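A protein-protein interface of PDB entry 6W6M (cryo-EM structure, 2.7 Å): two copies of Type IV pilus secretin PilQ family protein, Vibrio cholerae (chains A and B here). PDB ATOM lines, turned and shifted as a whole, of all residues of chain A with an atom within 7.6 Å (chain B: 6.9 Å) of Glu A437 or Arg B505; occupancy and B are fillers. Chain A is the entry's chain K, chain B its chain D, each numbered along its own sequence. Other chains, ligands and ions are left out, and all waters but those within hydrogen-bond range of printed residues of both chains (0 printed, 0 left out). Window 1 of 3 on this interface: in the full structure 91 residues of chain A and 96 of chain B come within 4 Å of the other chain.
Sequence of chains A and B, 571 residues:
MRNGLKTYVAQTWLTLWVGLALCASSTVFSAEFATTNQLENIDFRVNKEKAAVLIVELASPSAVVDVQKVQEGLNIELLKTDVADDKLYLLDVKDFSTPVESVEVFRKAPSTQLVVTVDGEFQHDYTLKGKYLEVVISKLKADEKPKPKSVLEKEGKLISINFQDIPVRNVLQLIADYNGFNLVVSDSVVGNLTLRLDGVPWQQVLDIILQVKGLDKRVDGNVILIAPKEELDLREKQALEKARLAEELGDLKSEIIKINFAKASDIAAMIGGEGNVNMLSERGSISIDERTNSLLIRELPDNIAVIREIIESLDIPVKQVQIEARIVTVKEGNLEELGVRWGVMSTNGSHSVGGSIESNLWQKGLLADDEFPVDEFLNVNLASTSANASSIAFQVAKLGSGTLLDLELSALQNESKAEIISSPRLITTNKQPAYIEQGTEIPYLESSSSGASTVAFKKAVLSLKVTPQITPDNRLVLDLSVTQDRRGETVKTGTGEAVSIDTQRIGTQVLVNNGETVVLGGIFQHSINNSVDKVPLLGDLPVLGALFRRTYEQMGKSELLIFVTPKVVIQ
The guanidinium group (NH1) of Arg B505 lies within salt-bridge range of the side-chain carboxylate (OE2) of Glu A441, at 2.8 Å. O of Arg B505 lies within hydrogen-bond range of N of Glu A437 (3.1 Å). N of Glu A441 sits at hydrogen-bond distance from O of Ile B501 (2.8 Å). N of Thr B503 sits at hydrogen-bond distance from O of Gly A439 (3.0 Å). The side-chain amide nitrogen of Gln B504 lies within hydrogen-bond range of the side-chain amide oxygen of Gln A438 (3.2 Å). O of Tyr A435 is in hydrogen-bond range of N of Gly B507.
The backbone NH of Leu A464 sits at hydrogen-bond distance from the backbone carbonyl oxygen of Ile A436 (3.0 Å). The backbone NH (N) of Leu A462 sits at hydrogen-bond distance from the backbone carbonyl oxygen (O) of Gln A438, at 2.9 Å. The backbone NH (N) of Gln B484 lies within hydrogen-bond range of the backbone carbonyl oxygen (O) of Gln B504 (3.0 Å). The backbone carbonyl oxygen (O) of Ile B506 is in hydrogen-bond range of the backbone NH (N) of Val B482 (3.0 Å). The guanidinium group of Arg B505 is in salt-bridge range of the side-chain carboxylate of Asp B485 (3.5 Å). The backbone carbonyl oxygen (O) of Ile B523 lies within hydrogen-bond range of the backbone NH (N) of Leu B560 (2.9 Å).
CB of Pro A424 touches CG1 of Ile B523, 3.9 Å away. Ile B506 touches Leu A426 (CD1 to CD2, 3.98 Å). Ile B506 touches Tyr A435 (CA to O, 3.7 Å). Ile A436 touches Arg B505. Ile A436 touches Ile B506 (CD1 to CD1, 3.9 Å). CA of Gln B504 touches O of Glu A437 (3.6 Å). O of Thr B503 touches CA of Gln A438 (3.5 Å). Gln A438 touches Ile B523 (CB to CD1, 3.8 Å). Glu A441 touches Lys B458 (OE1 to CE, 3.7 Å). OE2 of Glu A441 touches CG2 of Thr B503, at 3.8 Å.
Of chain B, only Gln B504 (3.6 Å) and Arg B505 (3.1 Å) come within 4 Å of Glu A437. Of chain A, only Ile A436, Glu A437 and Glu A441 come within 4 Å of Arg B505. Printed residues of chain B within 4 Å of Pro A424: Ile B523. Printed residues of chain A within 4 Å of Ile B506: Leu A426, Tyr A435 and Ile A436. The nearest residue of chain B that does not touch Glu A437 is Ile B523 (4.4 Å). The nearest residue of chain A that does not touch Arg B505 is Tyr A435 (4.4 Å). The nearest printed residue of chain A that does not touch Ile B523 is Leu A462 (4.01 Å).
Printed residues of chain B that touch a printed residue of chain A: Lys B458, Ile B501, Thr B503, Gln B504, Arg B505, Ile B506, Gly B507 and Ile B523. Hydrophobic or aromatic side chains of chain B within 4 Å of the printed part of chain A: Ile B506 and Ile B523. Of the 15 printed residues of chain A, 8 touch a printed residue of chain B. Among the printed residues, Asp or Glu carboxylates within 4 Å of a Lys or Arg side-chain nitrogen of the other chain: Glu A441 with Arg B505.
Positions printed for both chains: 459 and 483. Of the 16 pairs that touch across the chains among the printed residues, none has its exchanged pair printed and touching as well.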
ATOM      1  N   PRO A 424      12.250  12.960 -15.712  1.00  0.00           N
ATOM      2  CA  PRO A 424      11.840  13.177 -14.314  1.00  0.00           C
ATOM      3  C   PRO A 424      12.805  14.037 -13.499  1.00  0.00           C
ATOM      4  O   PRO A 424      13.971  14.163 -13.855  1.00  0.00           O
ATOM      5  CB  PRO A 424      11.753  11.750 -13.764  1.00  0.00           C
ATOM      6  CG  PRO A 424      12.644  10.960 -14.612  1.00  0.00           C
ATOM      7  CD  PRO A 424      12.636  11.562 -15.964  1.00  0.00           C
ATOM      8  N   LEU A 426      13.781  15.484  -9.210  1.00  0.00           N
ATOM      9  CA  LEU A 426      13.596  15.309  -7.778  1.00  0.00           C
ATOM     10  C   LEU A 426      14.372  16.388  -7.052  1.00  0.00           C
ATOM     11  O   LEU A 426      15.353  16.916  -7.567  1.00  0.00           O
ATOM     12  CB  LEU A 426      14.089  13.941  -7.308  1.00  0.00           C
ATOM     13  CG  LEU A 426      13.421  12.669  -7.776  1.00  0.00           C
ATOM     14  CD1 LEU A 426      14.213  11.517  -7.269  1.00  0.00           C
ATOM     15  CD2 LEU A 426      12.036  12.628  -7.241  1.00  0.00           C
ATOM     16  N   TYR A 435      13.009   8.726  -4.607  1.00  0.00           N
ATOM     17  CA  TYR A 435      12.525   8.063  -5.813  1.00  0.00           C
ATOM     18  C   TYR A 435      11.298   8.787  -6.352  1.00  0.00           C
ATOM     19  O   TYR A 435      10.555   9.416  -5.608  1.00  0.00           O
ATOM     20  CB  TYR A 435      12.197   6.583  -5.557  1.00  0.00           C
ATOM     21  CG  TYR A 435      11.089   6.381  -4.567  1.00  0.00           C
ATOM     22  CD1 TYR A 435       9.773   6.331  -4.981  1.00  0.00           C
ATOM     23  CD2 TYR A 435      11.357   6.222  -3.213  1.00  0.00           C
ATOM     24  CE1 TYR A 435       8.762   6.127  -4.086  1.00  0.00           C
ATOM     25  CE2 TYR A 435      10.352   6.014  -2.316  1.00  0.00           C
ATOM     26  CZ  TYR A 435       9.056   5.972  -2.757  1.00  0.00           C
ATOM     27  OH  TYR A 435       8.038   5.771  -1.867  1.00  0.00           O
ATOM     28  N   ILE A 436      11.098   8.681  -7.663  1.00  0.00           N
ATOM     29  CA  ILE A 436       9.860   9.115  -8.306  1.00  0.00           C
ATOM     30  C   ILE A 436       9.504   8.133  -9.421  1.00  0.00           C
ATOM     31  O   ILE A 436      10.383   7.671 -10.155  1.00  0.00           O
ATOM     32  CB  ILE A 436       9.953  10.571  -8.827  1.00  0.00           C
ATOM     33  CG1 ILE A 436       8.599  11.040  -9.357  1.00  0.00           C
ATOM     34  CG2 ILE A 436      11.026  10.738  -9.871  1.00  0.00           C
ATOM     35  CD1 ILE A 436       8.500  12.487  -9.596  1.00  0.00           C
ATOM     36  N   GLU A 437       8.210   7.810  -9.543  1.00  0.00           N
ATOM     37  CA  GLU A 437       7.718   6.722 -10.383  1.00  0.00           C
ATOM     38  C   GLU A 437       6.446   7.096 -11.127  1.00  0.00           C
ATOM     39  O   GLU A 437       5.691   7.961 -10.696  1.00  0.00           O
ATOM     40  CB  GLU A 437       7.390   5.482  -9.569  1.00  0.00           C
ATOM     41  CG  GLU A 437       8.531   4.601  -9.255  1.00  0.00           C
ATOM     42  CD  GLU A 437       8.110   3.472  -8.362  1.00  0.00           C
ATOM     43  OE1 GLU A 437       6.995   3.555  -7.816  1.00  0.00           O
ATOM     44  OE2 GLU A 437       8.880   2.501  -8.202  1.00  0.00           O
ATOM     45  N   GLN A 438       6.193   6.392 -12.229  1.00  0.00           N
ATOM     46  CA  GLN A 438       4.949   6.531 -12.983  1.00  0.00           C
ATOM     47  C   GLN A 438       4.782   5.311 -13.881  1.00  0.00           C
ATOM     48  O   GLN A 438       5.615   5.082 -14.759  1.00  0.00           O
ATOM     49  CB  GLN A 438       4.964   7.802 -13.804  1.00  0.00           C
ATOM     50  CG  GLN A 438       3.642   8.148 -14.400  1.00  0.00           C
ATOM     51  CD  GLN A 438       3.738   9.245 -15.416  1.00  0.00           C
ATOM     52  OE1 GLN A 438       3.054  10.253 -15.317  1.00  0.00           O
ATOM     53  NE2 GLN A 438       4.592   9.061 -16.402  1.00  0.00           N
ATOM     54  N   GLY A 439       3.722   4.538 -13.687  1.00  0.00           N
ATOM     55  CA  GLY A 439       3.520   3.373 -14.531  1.00  0.00           C
ATOM     56  C   GLY A 439       2.380   2.464 -14.138  1.00  0.00           C
ATOM     57  O   GLY A 439       1.316   2.949 -13.771  1.00  0.00           O
ATOM     58  N   GLU A 441       1.294  -1.639 -12.267  1.00  0.00           N
ATOM     59  CA  GLU A 441       1.686  -2.793 -11.463  1.00  0.00           C
ATOM     60  C   GLU A 441       0.913  -4.012 -11.940  1.00  0.00           C
ATOM     61  O   GLU A 441      -0.316  -4.038 -11.857  1.00  0.00           O
ATOM     62  CB  GLU A 441       1.427  -2.544  -9.982  1.00  0.00           C
ATOM     63  CG  GLU A 441       2.168  -1.369  -9.417  1.00  0.00           C
ATOM     64  CD  GLU A 441       1.960  -1.240  -7.936  1.00  0.00           C
ATOM     65  OE1 GLU A 441       1.089  -1.956  -7.409  1.00  0.00           O
ATOM     66  OE2 GLU A 441       2.668  -0.433  -7.296  1.00  0.00           O
ATOM     67  N   LYS A 459       6.471  -4.428 -11.389  1.00  0.00           N
ATOM     68  CA  LYS A 459       6.320  -3.040 -11.786  1.00  0.00           C
ATOM     69  C   LYS A 459       6.740  -2.835 -13.230  1.00  0.00           C
ATOM     70  O   LYS A 459       7.683  -3.466 -13.708  1.00  0.00           O
ATOM     71  CB  LYS A 459       7.135  -2.127 -10.883  1.00  0.00           C
ATOM     72  CG  LYS A 459       6.674  -2.116  -9.460  1.00  0.00           C
ATOM     73  CD  LYS A 459       7.500  -1.151  -8.654  1.00  0.00           C
ATOM     74  CE  LYS A 459       7.084  -1.157  -7.203  1.00  0.00           C
ATOM     75  NZ  LYS A 459       7.989  -0.324  -6.375  1.00  0.00           N
ATOM     76  N   VAL A 461       7.302   0.699 -14.867  1.00  0.00           N
ATOM     77  CA  VAL A 461       7.261   2.116 -14.544  1.00  0.00           C
ATOM     78  C   VAL A 461       8.403   2.836 -15.246  1.00  0.00           C
ATOM     79  O   VAL A 461       9.373   2.232 -15.690  1.00  0.00           O
ATOM     80  CB  VAL A 461       7.339   2.372 -13.022  1.00  0.00           C
ATOM     81  CG1 VAL A 461       6.139   1.800 -12.318  1.00  0.00           C
ATOM     82  CG2 VAL A 461       8.607   1.790 -12.454  1.00  0.00           C
ATOM     83  N   LEU A 462       8.238   4.151 -15.399  1.00  0.00           N
ATOM     84  CA  LEU A 462       9.374   5.064 -15.688  1.00  0.00           C
ATOM     85  C   LEU A 462       9.845   5.692 -14.373  1.00  0.00           C
ATOM     86  O   LEU A 462       9.105   6.516 -13.820  1.00  0.00           O
ATOM     87  CB  LEU A 462       8.899   6.135 -16.675  1.00  0.00           C
ATOM     88  CG  LEU A 462       9.713   7.427 -16.697  1.00  0.00           C
ATOM     89  CD1 LEU A 462      10.964   7.267 -17.543  1.00  0.00           C
ATOM     90  CD2 LEU A 462       8.869   8.583 -17.209  1.00  0.00           C
ATOM     91  N   SER A 463      11.026   5.297 -13.889  1.00  0.00           N
ATOM     92  CA  SER A 463      11.411   5.605 -12.524  1.00  0.00           C
ATOM     93  C   SER A 463      12.821   6.156 -12.423  1.00  0.00           C
ATOM     94  O   SER A 463      13.708   5.803 -13.204  1.00  0.00           O
ATOM     95  CB  SER A 463      11.301   4.380 -11.631  1.00  0.00           C
ATOM     96  OG  SER A 463      12.199   3.371 -12.026  1.00  0.00           O
ATOM     97  N   LEU A 464      13.009   7.013 -11.423  1.00  0.00           N
ATOM     98  CA  LEU A 464      14.312   7.520 -11.025  1.00  0.00           C
ATOM     99  C   LEU A 464      14.531   7.256  -9.545  1.00  0.00           C
ATOM    100  O   LEU A 464      13.671   7.564  -8.721  1.00  0.00           O
ATOM    101  CB  LEU A 464      14.433   9.012 -11.313  1.00  0.00           C
ATOM    102  CG  LEU A 464      15.721   9.709 -10.885  1.00  0.00           C
ATOM    103  CD1 LEU A 464      16.917   9.152 -11.617  1.00  0.00           C
ATOM    104  CD2 LEU A 464      15.611  11.194 -11.102  1.00  0.00           C
ATOM    105  N   LYS A 465      15.695   6.700  -9.215  1.00  0.00           N
ATOM    106  CA  LYS A 465      16.056   6.339  -7.848  1.00  0.00           C
ATOM    107  C   LYS A 465      17.471   6.820  -7.584  1.00  0.00           C
ATOM    108  O   LYS A 465      18.396   6.397  -8.285  1.00  0.00           O
ATOM    109  CB  LYS A 465      15.978   4.836  -7.671  1.00  0.00           C
ATOM    110  CG  LYS A 465      15.283   4.380  -6.441  1.00  0.00           C
ATOM    111  CD  LYS A 465      14.978   2.919  -6.553  1.00  0.00           C
ATOM    112  CE  LYS A 465      14.232   2.644  -7.833  1.00  0.00           C
ATOM    113  NZ  LYS A 465      13.014   3.490  -7.950  1.00  0.00           N
ATOM    114  N   THR A 483      15.075   3.768 -14.951  1.00  0.00           N
ATOM    115  CA  THR A 483      14.459   2.736 -15.778  1.00  0.00           C
ATOM    116  C   THR A 483      13.269   3.289 -16.545  1.00  0.00           C
ATOM    117  O   THR A 483      12.673   4.294 -16.168  1.00  0.00           O
ATOM    118  CB  THR A 483      13.977   1.512 -14.966  1.00  0.00           C
ATOM    119  OG1 THR A 483      12.660   1.742 -14.464  1.00  0.00           O
ATOM    120  CG2 THR A 483      14.892   1.206 -13.808  1.00  0.00           C
ATOM    121  N   LYS B 458      -5.281  -4.697  -1.848  1.00  0.00           N
ATOM    122  CA  LYS B 458      -4.294  -3.751  -2.333  1.00  0.00           C
ATOM    123  C   LYS B 458      -5.027  -2.405  -2.414  1.00  0.00           C
ATOM    124  O   LYS B 458      -6.244  -2.361  -2.585  1.00  0.00           O
ATOM    125  CB  LYS B 458      -3.752  -4.167  -3.696  1.00  0.00           C
ATOM    126  CG  LYS B 458      -2.730  -3.196  -4.260  1.00  0.00           C
ATOM    127  CD  LYS B 458      -1.504  -3.095  -3.372  1.00  0.00           C
ATOM    128  CE  LYS B 458      -0.420  -2.257  -4.029  1.00  0.00           C
ATOM    129  NZ  LYS B 458       0.704  -1.962  -3.100  1.00  0.00           N
ATOM    130  N   LYS B 459      -4.296  -1.305  -2.305  1.00  0.00           N
ATOM    131  CA  LYS B 459      -4.917   0.009  -2.298  1.00  0.00           C
ATOM    132  C   LYS B 459      -4.676   0.735  -3.609  1.00  0.00           C
ATOM    133  O   LYS B 459      -3.609   0.610  -4.212  1.00  0.00           O
ATOM    134  CB  LYS B 459      -4.389   0.849  -1.144  1.00  0.00           C
ATOM    135  CG  LYS B 459      -4.741   0.310   0.206  1.00  0.00           C
ATOM    136  CD  LYS B 459      -4.227   1.229   1.282  1.00  0.00           C
ATOM    137  CE  LYS B 459      -4.529   0.681   2.655  1.00  0.00           C
ATOM    138  NZ  LYS B 459      -3.897   1.500   3.718  1.00  0.00           N
ATOM    139  N   SER B 481       5.394  11.230   1.875  1.00  0.00           N
ATOM    140  CA  SER B 481       4.931  10.300   0.811  1.00  0.00           C
ATOM    141  C   SER B 481       3.644  10.840   0.182  1.00  0.00           C
ATOM    142  O   SER B 481       2.687  11.088   0.929  1.00  0.00           O
ATOM    143  CB  SER B 481       4.725   8.916   1.363  1.00  0.00           C
ATOM    144  OG  SER B 481       5.578   7.984   0.719  1.00  0.00           O
ATOM    145  N   VAL B 482       3.629  11.012  -1.140  1.00  0.00           N
ATOM    146  CA  VAL B 482       2.391  11.483  -1.840  1.00  0.00           C
ATOM    147  C   VAL B 482       2.104  10.564  -3.035  1.00  0.00           C
ATOM    148  O   VAL B 482       2.989  10.448  -3.898  1.00  0.00           O
ATOM    149  CB  VAL B 482       2.554  12.940  -2.313  1.00  0.00           C
ATOM    150  CG1 VAL B 482       1.323  13.445  -3.045  1.00  0.00           C
ATOM    151  CG2 VAL B 482       2.927  13.874  -1.173  1.00  0.00           C
ATOM    152  N   THR B 483       0.924   9.924  -3.090  1.00  0.00           N
ATOM    153  CA  THR B 483       0.629   9.019  -4.196  1.00  0.00           C
ATOM    154  C   THR B 483      -0.720   9.338  -4.818  1.00  0.00           C
ATOM    155  O   THR B 483      -1.588   9.943  -4.192  1.00  0.00           O
ATOM    156  CB  THR B 483       0.624   7.530  -3.782  1.00  0.00           C
ATOM    157  OG1 THR B 483      -0.664   7.162  -3.283  1.00  0.00           O
ATOM    158  CG2 THR B 483       1.658   7.233  -2.726  1.00  0.00           C
ATOM    159  N   GLN B 484      -0.893   8.876  -6.054  1.00  0.00           N
ATOM    160  CA  GLN B 484      -2.162   8.982  -6.768  1.00  0.00           C
ATOM    161  C   GLN B 484      -2.323   7.792  -7.705  1.00  0.00           C
ATOM    162  O   GLN B 484      -1.874   7.853  -8.847  1.00  0.00           O
ATOM    163  CB  GLN B 484      -2.221  10.276  -7.551  1.00  0.00           C
ATOM    164  CG  GLN B 484      -3.573  10.575  -8.091  1.00  0.00           C
ATOM    165  CD  GLN B 484      -3.593  11.818  -8.912  1.00  0.00           C
ATOM    166  OE1 GLN B 484      -4.608  12.487  -9.003  1.00  0.00           O
ATOM    167  NE2 GLN B 484      -2.468  12.140  -9.518  1.00  0.00           N
ATOM    168  N   ASP B 485      -2.993   6.737  -7.255  1.00  0.00           N
ATOM    169  CA  ASP B 485      -3.173   5.517  -8.034  1.00  0.00           C
ATOM    170  C   ASP B 485      -4.629   5.350  -8.450  1.00  0.00           C
ATOM    171  O   ASP B 485      -5.537   5.930  -7.867  1.00  0.00           O
ATOM    172  CB  ASP B 485      -2.730   4.287  -7.248  1.00  0.00           C
ATOM    173  CG  ASP B 485      -1.431   4.495  -6.529  1.00  0.00           C
ATOM    174  OD1 ASP B 485      -0.542   5.177  -7.067  1.00  0.00           O
ATOM    175  OD2 ASP B 485      -1.296   3.974  -5.407  1.00  0.00           O
ATOM    176  N   ILE B 501      -3.066  -2.006 -11.658  1.00  0.00           N
ATOM    177  CA  ILE B 501      -3.138  -0.692 -11.028  1.00  0.00           C
ATOM    178  C   ILE B 501      -2.191   0.260 -11.739  1.00  0.00           C
ATOM    179  O   ILE B 501      -1.078  -0.126 -12.101  1.00  0.00           O
ATOM    180  CB  ILE B 501      -2.799  -0.788  -9.524  1.00  0.00           C
ATOM    181  CG1 ILE B 501      -3.870  -1.596  -8.797  1.00  0.00           C
ATOM    182  CG2 ILE B 501      -2.664   0.578  -8.899  1.00  0.00           C
ATOM    183  CD1 ILE B 501      -3.516  -1.970  -7.397  1.00  0.00           C
ATOM    184  N   THR B 503      -0.105   3.841 -11.325  1.00  0.00           N
ATOM    185  CA  THR B 503       0.440   4.535 -10.165  1.00  0.00           C
ATOM    186  C   THR B 503       1.224   5.788 -10.537  1.00  0.00           C
ATOM    187  O   THR B 503       1.722   5.924 -11.651  1.00  0.00           O
ATOM    188  CB  THR B 503       1.359   3.599  -9.336  1.00  0.00           C
ATOM    189  OG1 THR B 503       2.439   3.120 -10.144  1.00  0.00           O
ATOM    190  CG2 THR B 503       0.586   2.414  -8.812  1.00  0.00           C
ATOM    191  N   GLN B 504       1.302   6.714  -9.578  1.00  0.00           N
ATOM    192  CA  GLN B 504       2.252   7.824  -9.538  1.00  0.00           C
ATOM    193  C   GLN B 504       2.668   8.008  -8.093  1.00  0.00           C
ATOM    194  O   GLN B 504       1.807   8.132  -7.228  1.00  0.00           O
ATOM    195  CB  GLN B 504       1.655   9.131 -10.040  1.00  0.00           C
ATOM    196  CG  GLN B 504       1.321   9.153 -11.478  1.00  0.00           C
ATOM    197  CD  GLN B 504       0.671  10.445 -11.881  1.00  0.00           C
ATOM    198  OE1 GLN B 504       0.069  11.123 -11.065  1.00  0.00           O
ATOM    199  NE2 GLN B 504       0.793  10.795 -13.146  1.00  0.00           N
ATOM    200  N   ARG B 505       3.966   8.024  -7.822  1.00  0.00           N
ATOM    201  CA  ARG B 505       4.439   8.023  -6.448  1.00  0.00           C
ATOM    202  C   ARG B 505       5.677   8.887  -6.312  1.00  0.00           C
ATOM    203  O   ARG B 505       6.514   8.952  -7.206  1.00  0.00           O
ATOM    204  CB  ARG B 505       4.753   6.606  -5.967  1.00  0.00           C
ATOM    205  CG  ARG B 505       3.538   5.784  -5.708  1.00  0.00           C
ATOM    206  CD  ARG B 505       3.843   4.330  -5.505  1.00  0.00           C
ATOM    207  NE  ARG B 505       2.600   3.578  -5.392  1.00  0.00           N
ATOM    208  CZ  ARG B 505       2.512   2.254  -5.370  1.00  0.00           C
ATOM    209  NH1 ARG B 505       3.601   1.510  -5.455  1.00  0.00           N
ATOM    210  NH2 ARG B 505       1.327   1.673  -5.274  1.00  0.00           N
ATOM    211  N   ILE B 506       5.796   9.534  -5.160  1.00  0.00           N
ATOM    212  CA  ILE B 506       7.008  10.259  -4.817  1.00  0.00           C
ATOM    213  C   ILE B 506       7.188  10.199  -3.309  1.00  0.00           C
ATOM    214  O   ILE B 506       6.238  10.373  -2.542  1.00  0.00           O
ATOM    215  CB  ILE B 506       6.970  11.707  -5.359  1.00  0.00           C
ATOM    216  CG1 ILE B 506       8.302  12.401  -5.121  1.00  0.00           C
ATOM    217  CG2 ILE B 506       5.846  12.506  -4.759  1.00  0.00           C
ATOM    218  CD1 ILE B 506       8.443  13.656  -5.868  1.00  0.00           C
ATOM    219  N   GLY B 507       8.414   9.916  -2.897  1.00  0.00           N
ATOM    220  CA  GLY B 507       8.776   9.855  -1.499  1.00  0.00           C
ATOM    221  C   GLY B 507      10.110  10.511  -1.231  1.00  0.00           C
ATOM    222  O   GLY B 507      11.088  10.209  -1.906  1.00  0.00           O
ATOM    223  N   ILE B 523       7.422  15.210 -13.906  1.00  0.00           N
ATOM    224  CA  ILE B 523       7.783  14.406 -15.070  1.00  0.00           C
ATOM    225  C   ILE B 523       7.296  15.124 -16.316  1.00  0.00           C
ATOM    226  O   ILE B 523       6.166  15.614 -16.357  1.00  0.00           O
ATOM    227  CB  ILE B 523       7.210  12.976 -15.003  1.00  0.00           C
ATOM    228  CG1 ILE B 523       7.838  12.193 -13.860  1.00  0.00           C
ATOM    229  CG2 ILE B 523       7.472  12.233 -16.291  1.00  0.00           C
ATOM    230  CD1 ILE B 523       7.167  10.900 -13.560  1.00  0.00           C
ATOM    231  N   LEU B 560       3.639  16.736 -15.492  1.00  0.00           N
ATOM    232  CA  LEU B 560       3.146  16.491 -14.114  1.00  0.00           C
ATOM    233  C   LEU B 560       4.050  17.230 -13.126  1.00  0.00           C
ATOM    234  O   LEU B 560       5.274  17.234 -13.335  1.00  0.00           O
ATOM    235  CB  LEU B 560       3.156  14.982 -13.846  1.00  0.00           C
ATOM    236  CG  LEU B 560       3.241  14.579 -12.376  1.00  0.00           C
ATOM    237  CD1 LEU B 560       1.857  14.504 -11.755  1.00  0.00           C
ATOM    238  CD2 LEU B 560       3.967  13.253 -12.218  1.00  0.00           C
ATOM    239  N   ILE B 562       4.438  18.300  -8.676  1.00  0.00           N
ATOM    240  CA  ILE B 562       3.993  18.116  -7.296  1.00  0.00           C
ATOM    241  C   ILE B 562       4.559  19.227  -6.419  1.00  0.00           C
ATOM    242  O   ILE B 562       5.771  19.448  -6.399  1.00  0.00           O
ATOM    243  CB  ILE B 562       4.400  16.734  -6.756  1.00  0.00           C
ATOM    244  CG1 ILE B 562       3.657  15.634  -7.515  1.00  0.00           C
ATOM    245  CG2 ILE B 562       4.094  16.634  -5.285  1.00  0.00           C
ATOM    246  CD1 ILE B 562       4.155  14.257  -7.262  1.00  0.00           C
